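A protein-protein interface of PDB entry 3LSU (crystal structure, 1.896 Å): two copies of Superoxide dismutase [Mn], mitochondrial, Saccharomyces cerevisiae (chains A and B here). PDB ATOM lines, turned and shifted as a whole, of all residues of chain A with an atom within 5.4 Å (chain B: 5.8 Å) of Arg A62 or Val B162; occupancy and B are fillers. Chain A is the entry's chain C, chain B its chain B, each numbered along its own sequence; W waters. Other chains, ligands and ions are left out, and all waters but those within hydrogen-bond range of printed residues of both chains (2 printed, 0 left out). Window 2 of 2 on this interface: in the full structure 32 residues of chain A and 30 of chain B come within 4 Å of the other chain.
The backbone carbonyl oxygen (O) of Val B157 lies within hydrogen-bond range of the guanidinium group (NE) of Arg A62 (2.8 Å). The guanidinium group (NH2) of Arg A62 is in hydrogen-bond range of the backbone carbonyl oxygen (O) of Gly B159 (3.0 Å). The backbone carbonyl oxygen of Leu B161 sits at hydrogen-bond distance from the guanidinium group of Arg A62.
O of Val B162 lies within hydrogen-bond range of N of MLY B138, at 2.9 Å.
Pro A58 touches Thr B79 (O to OG1, 3.97 Å). Ala A61 touches Thr B79 (CB to OG1, 3.4 Å). C of Thr B158 touches NH2 of Arg A62, at 3.4 Å. Arg A62 touches Val B162 (NH2 to CA, 3.8 Å). CD of Pro B163 touches NE of Arg A62, at 3.9 Å. CD of Arg A62 touches CD1 of Ile B207 (3.4 Å). CD1 of Ile A65 touches OG1 of Thr B79, at 3.7 Å. Thr B158 touches Ala A66.
Arg A62 touches just these residues of chain B: Val B157, Thr B158, Gly B159, Leu B161, Val B162, Pro B163 and Ile B207. Of the printed residues of chain B, Ile A65 touches Thr B79. Of the printed residues of chain A, Thr B79 touches Pro A58, Ala A61 and Ile A65. Thr B156 touches none of the printed residues of chain A. Of the printed residues of chain A, Thr B158 touches Arg A62 and Ala A66. Val B162 touches just one residue of chain A: Arg A62 (3.8 Å).
Of the 10 printed residues of chain A, 5 touch a printed residue of chain B. Hydrophobic or aromatic side chains of chain A that line the printed part of chain B: Ala A61, Ile A65 and Ala A66. Of the 19 printed residues of chain B, 8 touch a printed residue of chain A. Printed residues of chain B that touch a printed residue of chain A: Thr B79, Val B157, Thr B158, Gly B159, Leu B161, Val B162, Pro B163 and Ile B207. Hydrophobic or aromatic side chains of chain B within 4 Å of the printed part of chain A: Pro B163 and Ile B207. Along chain B the printed residues that touch a printed residue of chain A span positions 79 to 207. Among the printed residues, 11 pairs touch across the chains. Among the printed residues, no Asp or Glu carboxylate lies within 4 Å of a Lys or Arg side-chain nitrogen of the other chain.
No position is printed for both chains.
Water W1 lies within hydrogen-bond range of the backbone carbonyl oxygen (O) of Gly B159 (2.6 Å) and the guanidinium group (NH1) of Arg A62 (2.9 Å). Water W2 lies within hydrogen-bond range of OG1 of Thr B156 (2.8 Å), O of Val B157 (2.9 Å) and NE of Arg A62 (3.4 Å).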
ATOM      1  N   SER A  57     -35.077   8.385 -21.780  1.00  0.00           N
ATOM      2  CA  SER A  57     -33.796   8.578 -21.103  1.00  0.00           C
ATOM      3  C   SER A  57     -33.345   7.293 -20.404  1.00  0.00           C
ATOM      4  O   SER A  57     -34.160   6.423 -20.101  1.00  0.00           O
ATOM      5  CB  SER A  57     -33.943   9.677 -20.042  1.00  0.00           C
ATOM      6  OG  SER A  57     -34.920   9.291 -19.081  1.00  0.00           O
ATOM      7  N   PRO A  58     -32.037   7.169 -20.146  1.00  0.00           N
ATOM      8  CA  PRO A  58     -31.562   6.086 -19.281  1.00  0.00           C
ATOM      9  C   PRO A  58     -32.253   6.134 -17.912  1.00  0.00           C
ATOM     10  O   PRO A  58     -32.522   5.082 -17.332  1.00  0.00           O
ATOM     11  CB  PRO A  58     -30.064   6.381 -19.152  1.00  0.00           C
ATOM     12  CG  PRO A  58     -29.715   7.075 -20.440  1.00  0.00           C
ATOM     13  CD  PRO A  58     -30.928   7.912 -20.775  1.00  0.00           C
ATOM     14  N   ALA A  59     -32.538   7.332 -17.403  1.00  0.00           N
ATOM     15  CA  ALA A  59     -33.262   7.456 -16.131  1.00  0.00           C
ATOM     16  C   ALA A  59     -34.596   6.709 -16.163  1.00  0.00           C
ATOM     17  O   ALA A  59     -34.924   5.958 -15.246  1.00  0.00           O
ATOM     18  CB  ALA A  59     -33.488   8.930 -15.759  1.00  0.00           C
ATOM     19  N   ASN A  60     -35.367   6.915 -17.222  1.00  0.00           N
ATOM     20  CA  ASN A  60     -36.653   6.240 -17.337  1.00  0.00           C
ATOM     21  C   ASN A  60     -36.522   4.765 -17.714  1.00  0.00           C
ATOM     22  O   ASN A  60     -37.327   3.938 -17.290  1.00  0.00           O
ATOM     23  CB  ASN A  60     -37.577   6.997 -18.294  1.00  0.00           C
ATOM     24  CG  ASN A  60     -37.988   8.345 -17.734  1.00  0.00           C
ATOM     25  OD1 ASN A  60     -38.066   8.514 -16.516  1.00  0.00           O
ATOM     26  ND2 ASN A  60     -38.246   9.306 -18.609  1.00  0.00           N
ATOM     27  N   ALA A  61     -35.510   4.435 -18.507  1.00  0.00           N
ATOM     28  CA  ALA A  61     -35.209   3.034 -18.799  1.00  0.00           C
ATOM     29  C   ALA A  61     -34.926   2.299 -17.490  1.00  0.00           C
ATOM     30  O   ALA A  61     -35.395   1.182 -17.270  1.00  0.00           O
ATOM     31  CB  ALA A  61     -34.011   2.923 -19.751  1.00  0.00           C
ATOM     32  N   ARG A  62     -34.160   2.950 -16.620  1.00  0.00           N
ATOM     33  CA  ARG A  62     -33.807   2.395 -15.316  1.00  0.00           C
ATOM     34  C   ARG A  62     -35.058   2.098 -14.483  1.00  0.00           C
ATOM     35  O   ARG A  62     -35.153   1.060 -13.828  1.00  0.00           O
ATOM     36  CB  ARG A  62     -32.860   3.373 -14.597  1.00  0.00           C
ATOM     37  CG  ARG A  62     -32.244   2.897 -13.296  1.00  0.00           C
ATOM     38  CD  ARG A  62     -31.116   3.855 -12.894  1.00  0.00           C
ATOM     39  NE  ARG A  62     -30.633   3.636 -11.539  1.00  0.00           N
ATOM     40  CZ  ARG A  62     -31.051   4.324 -10.481  1.00  0.00           C
ATOM     41  NH1 ARG A  62     -31.966   5.278 -10.626  1.00  0.00           N
ATOM     42  NH2 ARG A  62     -30.557   4.060  -9.280  1.00  0.00           N
ATOM     43  N   MLY A  63     -36.029   3.007 -14.515  1.00  0.00           N
ATOM     44  CA  MLY A  63     -37.269   2.783 -13.786  1.00  0.00           C
ATOM     45  CB  MLY A  63     -38.161   4.055 -13.793  1.00  0.00           C
ATOM     46  CG  MLY A  63     -37.548   5.347 -13.137  1.00  0.00           C
ATOM     47  CD  MLY A  63     -38.411   6.672 -13.273  1.00  0.00           C
ATOM     48  CE  MLY A  63     -38.347   7.645 -12.107  1.00  0.00           C
ATOM     49  NZ  MLY A  63     -38.566   9.084 -12.367  1.00  0.00           N
ATOM     50  CH1 MLY A  63     -37.673   9.857 -11.517  1.00  0.00           C
ATOM     51  CH2 MLY A  63     -38.276   9.390 -13.777  1.00  0.00           C
ATOM     52  C   MLY A  63     -38.059   1.572 -14.329  1.00  0.00           C
ATOM     53  O   MLY A  63     -38.634   0.842 -13.603  1.00  0.00           O
ATOM     54  N   MET A  64     -38.071   1.439 -15.651  1.00  0.00           N
ATOM     55  CA  MET A  64     -38.728   0.327 -16.332  1.00  0.00           C
ATOM     56  C   MET A  64     -38.097  -1.009 -15.926  1.00  0.00           C
ATOM     57  O   MET A  64     -38.797  -1.969 -15.600  1.00  0.00           O
ATOM     58  CB  MET A  64     -38.646   0.547 -17.850  1.00  0.00           C
ATOM     59  CG  MET A  64     -39.186  -0.586 -18.701  1.00  0.00           C
ATOM     60  SD  MET A  64     -40.946  -0.850 -18.462  1.00  0.00           S
ATOM     61  CE  MET A  64     -41.629   0.540 -19.392  1.00  0.00           C
ATOM     62  N   ILE A  65     -36.769  -1.054 -15.915  1.00  0.00           N
ATOM     63  CA  ILE A  65     -36.037  -2.243 -15.480  1.00  0.00           C
ATOM     64  C   ILE A  65     -36.419  -2.623 -14.047  1.00  0.00           C
ATOM     65  O   ILE A  65     -36.637  -3.794 -13.735  1.00  0.00           O
ATOM     66  CB  ILE A  65     -34.512  -1.995 -15.540  1.00  0.00           C
ATOM     67  CG1 ILE A  65     -34.065  -1.712 -16.980  1.00  0.00           C
ATOM     68  CG2 ILE A  65     -33.740  -3.155 -14.924  1.00  0.00           C
ATOM     69  CD1 ILE A  65     -32.655  -1.102 -17.061  1.00  0.00           C
ATOM     70  N   ALA A  66     -36.504  -1.622 -13.177  1.00  0.00           N
ATOM     71  CA  ALA A  66     -36.790  -1.870 -11.764  1.00  0.00           C
ATOM     72  C   ALA A  66     -38.126  -2.587 -11.494  1.00  0.00           C
ATOM     73  O   ALA A  66     -38.257  -3.283 -10.493  1.00  0.00           O
ATOM     74  CB  ALA A  66     -36.702  -0.564 -10.954  1.00  0.00           C
ATOM     75  N   THR B  79     -29.053   1.110 -20.865  1.00  0.00           N
ATOM     76  CA  THR B  79     -28.750   2.016 -19.754  1.00  0.00           C
ATOM     77  C   THR B  79     -27.280   2.015 -19.353  1.00  0.00           C
ATOM     78  O   THR B  79     -26.674   3.077 -19.177  1.00  0.00           O
ATOM     79  CB  THR B  79     -29.582   1.666 -18.505  1.00  0.00           C
ATOM     80  OG1 THR B  79     -30.976   1.742 -18.825  1.00  0.00           O
ATOM     81  CG2 THR B  79     -29.263   2.637 -17.351  1.00  0.00           C
ATOM     82  N   ILE B 136     -19.465   2.128  -9.094  1.00  0.00           N
ATOM     83  CA  ILE B 136     -19.312   2.903  -7.879  1.00  0.00           C
ATOM     84  C   ILE B 136     -20.632   3.639  -7.722  1.00  0.00           C
ATOM     85  O   ILE B 136     -21.084   4.316  -8.649  1.00  0.00           O
ATOM     86  CB  ILE B 136     -18.140   3.903  -8.004  1.00  0.00           C
ATOM     87  CG1 ILE B 136     -16.823   3.145  -8.194  1.00  0.00           C
ATOM     88  CG2 ILE B 136     -18.066   4.815  -6.782  1.00  0.00           C
ATOM     89  CD1 ILE B 136     -15.638   4.055  -8.546  1.00  0.00           C
ATOM     90  N   VAL B 137     -21.275   3.483  -6.570  1.00  0.00           N
ATOM     91  CA  VAL B 137     -22.621   4.000  -6.399  1.00  0.00           C
ATOM     92  C   VAL B 137     -22.717   4.892  -5.190  1.00  0.00           C
ATOM     93  O   VAL B 137     -21.882   4.836  -4.292  1.00  0.00           O
ATOM     94  CB  VAL B 137     -23.643   2.857  -6.193  1.00  0.00           C
ATOM     95  CG1 VAL B 137     -23.648   1.921  -7.403  1.00  0.00           C
ATOM     96  CG2 VAL B 137     -23.333   2.088  -4.907  1.00  0.00           C
ATOM     97  N   MLY B 138     -23.756   5.718  -5.180  1.00  0.00           N
ATOM     98  CA  MLY B 138     -24.158   6.398  -3.977  1.00  0.00           C
ATOM     99  CB  MLY B 138     -24.358   7.912  -4.241  1.00  0.00           C
ATOM    100  CG  MLY B 138     -24.914   8.732  -3.022  1.00  0.00           C
ATOM    101  CD  MLY B 138     -25.304  10.237  -3.304  1.00  0.00           C
ATOM    102  CE  MLY B 138     -25.493  11.033  -2.028  1.00  0.00           C
ATOM    103  NZ  MLY B 138     -25.838  12.470  -2.080  1.00  0.00           N
ATOM    104  CH1 MLY B 138     -24.626  13.235  -2.230  1.00  0.00           C
ATOM    105  CH2 MLY B 138     -26.837  12.766  -3.121  1.00  0.00           C
ATOM    106  C   MLY B 138     -25.470   5.761  -3.487  1.00  0.00           C
ATOM    107  O   MLY B 138     -26.426   5.719  -4.182  1.00  0.00           O
ATOM    108  N   ASN B 139     -25.445   5.244  -2.265  1.00  0.00           N
ATOM    109  CA  ASN B 139     -26.600   4.567  -1.691  1.00  0.00           C
ATOM    110  C   ASN B 139     -27.480   5.572  -0.934  1.00  0.00           C
ATOM    111  O   ASN B 139     -27.130   6.011   0.160  1.00  0.00           O
ATOM    112  CB  ASN B 139     -26.139   3.427  -0.766  1.00  0.00           C
ATOM    113  CG  ASN B 139     -27.298   2.607  -0.215  1.00  0.00           C
ATOM    114  OD1 ASN B 139     -28.470   2.974  -0.367  1.00  0.00           O
ATOM    115  ND2 ASN B 139     -26.976   1.493   0.429  1.00  0.00           N
ATOM    116  N   LEU B 140     -28.616   5.933  -1.526  1.00  0.00           N
ATOM    117  CA  LEU B 140     -29.516   6.918  -0.923  1.00  0.00           C
ATOM    118  C   LEU B 140     -30.234   6.391   0.313  1.00  0.00           C
ATOM    119  O   LEU B 140     -30.797   7.172   1.079  1.00  0.00           O
ATOM    120  CB  LEU B 140     -30.550   7.396  -1.945  1.00  0.00           C
ATOM    121  CG  LEU B 140     -30.017   7.858  -3.306  1.00  0.00           C
ATOM    122  CD1 LEU B 140     -31.188   8.158  -4.239  1.00  0.00           C
ATOM    123  CD2 LEU B 140     -29.132   9.082  -3.169  1.00  0.00           C
ATOM    124  N   THR B 156     -28.365  -4.059 -13.665  1.00  0.00           N
ATOM    125  CA  THR B 156     -27.866  -2.732 -13.336  1.00  0.00           C
ATOM    126  C   THR B 156     -28.306  -2.335 -11.933  1.00  0.00           C
ATOM    127  O   THR B 156     -29.028  -3.082 -11.270  1.00  0.00           O
ATOM    128  CB  THR B 156     -28.318  -1.680 -14.382  1.00  0.00           C
ATOM    129  OG1 THR B 156     -27.574  -0.464 -14.204  1.00  0.00           O
ATOM    130  CG2 THR B 156     -29.810  -1.393 -14.250  1.00  0.00           C
ATOM    131  N   VAL B 157     -27.861  -1.171 -11.472  1.00  0.00           N
ATOM    132  CA  VAL B 157     -28.226  -0.717 -10.143  1.00  0.00           C
ATOM    133  C   VAL B 157     -29.410   0.239 -10.246  1.00  0.00           C
ATOM    134  O   VAL B 157     -29.377   1.195 -11.019  1.00  0.00           O
ATOM    135  CB  VAL B 157     -27.029  -0.074  -9.403  1.00  0.00           C
ATOM    136  CG1 VAL B 157     -26.036  -1.146  -8.995  1.00  0.00           C
ATOM    137  CG2 VAL B 157     -26.359   0.986 -10.272  1.00  0.00           C
ATOM    138  N   THR B 158     -30.465  -0.051  -9.489  1.00  0.00           N
ATOM    139  CA  THR B 158     -31.718   0.691  -9.594  1.00  0.00           C
ATOM    140  C   THR B 158     -32.118   1.249  -8.235  1.00  0.00           C
ATOM    141  O   THR B 158     -31.475   0.961  -7.227  1.00  0.00           O
ATOM    142  CB  THR B 158     -32.862  -0.201 -10.132  1.00  0.00           C
ATOM    143  OG1 THR B 158     -33.032  -1.337  -9.271  1.00  0.00           O
ATOM    144  CG2 THR B 158     -32.544  -0.695 -11.544  1.00  0.00           C
ATOM    145  N   GLY B 159     -33.182   2.047  -8.215  1.00  0.00           N
ATOM    146  CA  GLY B 159     -33.737   2.560  -6.968  1.00  0.00           C
ATOM    147  C   GLY B 159     -32.746   3.414  -6.207  1.00  0.00           C
ATOM    148  O   GLY B 159     -32.176   4.359  -6.773  1.00  0.00           O
ATOM    149  N   PRO B 160     -32.508   3.074  -4.927  1.00  0.00           N
ATOM    150  CA  PRO B 160     -31.614   3.864  -4.070  1.00  0.00           C
ATOM    151  C   PRO B 160     -30.140   3.779  -4.480  1.00  0.00           C
ATOM    152  O   PRO B 160     -29.366   4.625  -4.046  1.00  0.00           O
ATOM    153  CB  PRO B 160     -31.794   3.246  -2.673  1.00  0.00           C
ATOM    154  CG  PRO B 160     -32.719   2.071  -2.838  1.00  0.00           C
ATOM    155  CD  PRO B 160     -32.934   1.816  -4.290  1.00  0.00           C
ATOM    156  N   LEU B 161     -29.754   2.801  -5.296  1.00  0.00           N
ATOM    157  CA  LEU B 161     -28.358   2.693  -5.701  1.00  0.00           C
ATOM    158  C   LEU B 161     -28.096   3.493  -6.973  1.00  0.00           C
ATOM    159  O   LEU B 161     -28.377   3.025  -8.077  1.00  0.00           O
ATOM    160  CB  LEU B 161     -27.946   1.228  -5.916  1.00  0.00           C
ATOM    161  CG  LEU B 161     -28.020   0.341  -4.670  1.00  0.00           C
ATOM    162  CD1 LEU B 161     -27.571  -1.093  -4.978  1.00  0.00           C
ATOM    163  CD2 LEU B 161     -27.203   0.945  -3.527  1.00  0.00           C
ATOM    164  N   VAL B 162     -27.551   4.696  -6.813  1.00  0.00           N
ATOM    165  CA  VAL B 162     -27.312   5.603  -7.935  1.00  0.00           C
ATOM    166  C   VAL B 162     -25.923   5.373  -8.504  1.00  0.00           C
ATOM    167  O   VAL B 162     -24.937   5.565  -7.807  1.00  0.00           O
ATOM    168  CB  VAL B 162     -27.408   7.091  -7.488  1.00  0.00           C
ATOM    169  CG1 VAL B 162     -27.184   8.027  -8.667  1.00  0.00           C
ATOM    170  CG2 VAL B 162     -28.760   7.375  -6.817  1.00  0.00           C
ATOM    171  N   PRO B 163     -25.839   4.969  -9.785  1.00  0.00           N
ATOM    172  CA  PRO B 163     -24.521   4.735 -10.378  1.00  0.00           C
ATOM    173  C   PRO B 163     -23.734   6.047 -10.554  1.00  0.00           C
ATOM    174  O   PRO B 163     -24.261   7.029 -11.074  1.00  0.00           O
ATOM    175  CB  PRO B 163     -24.860   4.102 -11.732  1.00  0.00           C
ATOM    176  CG  PRO B 163     -26.225   4.641 -12.068  1.00  0.00           C
ATOM    177  CD  PRO B 163     -26.939   4.721 -10.738  1.00  0.00           C
ATOM    178  N   LEU B 164     -22.487   6.058 -10.100  1.00  0.00           N
ATOM    179  CA  LEU B 164     -21.610   7.215 -10.267  1.00  0.00           C
ATOM    180  C   LEU B 164     -20.588   6.954 -11.378  1.00  0.00           C
ATOM    181  O   LEU B 164     -20.350   7.801 -12.249  1.00  0.00           O
ATOM    182  CB  LEU B 164     -20.892   7.518  -8.955  1.00  0.00           C
ATOM    183  CG  LEU B 164     -21.813   7.747  -7.743  1.00  0.00           C
ATOM    184  CD1 LEU B 164     -20.997   8.085  -6.516  1.00  0.00           C
ATOM    185  CD2 LEU B 164     -22.816   8.832  -8.017  1.00  0.00           C
ATOM    186  N   ARG B 201     -23.275  13.315 -10.971  1.00  0.00           N
ATOM    187  CA  ARG B 201     -24.208  12.270 -10.543  1.00  0.00           C
ATOM    188  C   ARG B 201     -24.301  12.176  -9.014  1.00  0.00           C
ATOM    189  O   ARG B 201     -25.384  11.953  -8.462  1.00  0.00           O
ATOM    190  CB  ARG B 201     -23.781  10.911 -11.111  1.00  0.00           C
ATOM    191  CG  ARG B 201     -23.885  10.822 -12.617  1.00  0.00           C
ATOM    192  CD  ARG B 201     -23.196   9.561 -13.117  1.00  0.00           C
ATOM    193  NE  ARG B 201     -23.265   9.448 -14.566  1.00  0.00           N
ATOM    194  CZ  ARG B 201     -22.633   8.504 -15.263  1.00  0.00           C
ATOM    195  NH1 ARG B 201     -21.884   7.599 -14.631  1.00  0.00           N
ATOM    196  NH2 ARG B 201     -22.752   8.466 -16.582  1.00  0.00           N
ATOM    197  N   GLY B 205     -27.716  13.010  -7.092  1.00  0.00           N
ATOM    198  CA  GLY B 205     -28.348  11.839  -6.507  1.00  0.00           C
ATOM    199  C   GLY B 205     -29.277  11.139  -7.481  1.00  0.00           C
ATOM    200  O   GLY B 205     -30.230  10.483  -7.079  1.00  0.00           O
ATOM    201  N   MLY B 206     -29.007  11.292  -8.772  1.00  0.00           N
ATOM    202  CA  MLY B 206     -29.793  10.626  -9.801  1.00  0.00           C
ATOM    203  CB  MLY B 206     -31.152  11.334 -10.063  1.00  0.00           C
ATOM    204  CG  MLY B 206     -31.042  12.854 -10.479  1.00  0.00           C
ATOM    205  CD  MLY B 206     -32.358  13.614 -10.916  1.00  0.00           C
ATOM    206  CE  MLY B 206     -32.169  14.898 -11.712  1.00  0.00           C
ATOM    207  NZ  MLY B 206     -33.356  15.755 -11.966  1.00  0.00           N
ATOM    208  CH1 MLY B 206     -33.094  17.068 -11.407  1.00  0.00           C
ATOM    209  CH2 MLY B 206     -34.546  15.182 -11.309  1.00  0.00           C
ATOM    210  C   MLY B 206     -28.971  10.589 -11.099  1.00  0.00           C
ATOM    211  O   MLY B 206     -27.944  11.171 -11.153  1.00  0.00           O
ATOM    212  N   ILE B 207     -29.461   9.896 -12.122  1.00  0.00           N
ATOM    213  CA  ILE B 207     -28.790   9.931 -13.421  1.00  0.00           C
ATOM    214  C   ILE B 207     -29.597  10.698 -14.467  1.00  0.00           C
ATOM    215  O   ILE B 207     -30.014  11.837 -14.227  1.00  0.00           O
ATOM    216  CB  ILE B 207     -28.479   8.522 -13.941  1.00  0.00           C
ATOM    217  CG1 ILE B 207     -29.743   7.659 -13.894  1.00  0.00           C
ATOM    218  CG2 ILE B 207     -27.348   7.914 -13.123  1.00  0.00           C
ATOM    219  CD1 ILE B 207     -29.639   6.371 -14.696  1.00  0.00           C
HETATM  220  O   HOH W   1     -33.062   6.320  -8.154  1.00  0.00           O
HETATM  221  O   HOH W   2     -28.450   2.125 -13.603  1.00  0.00           O
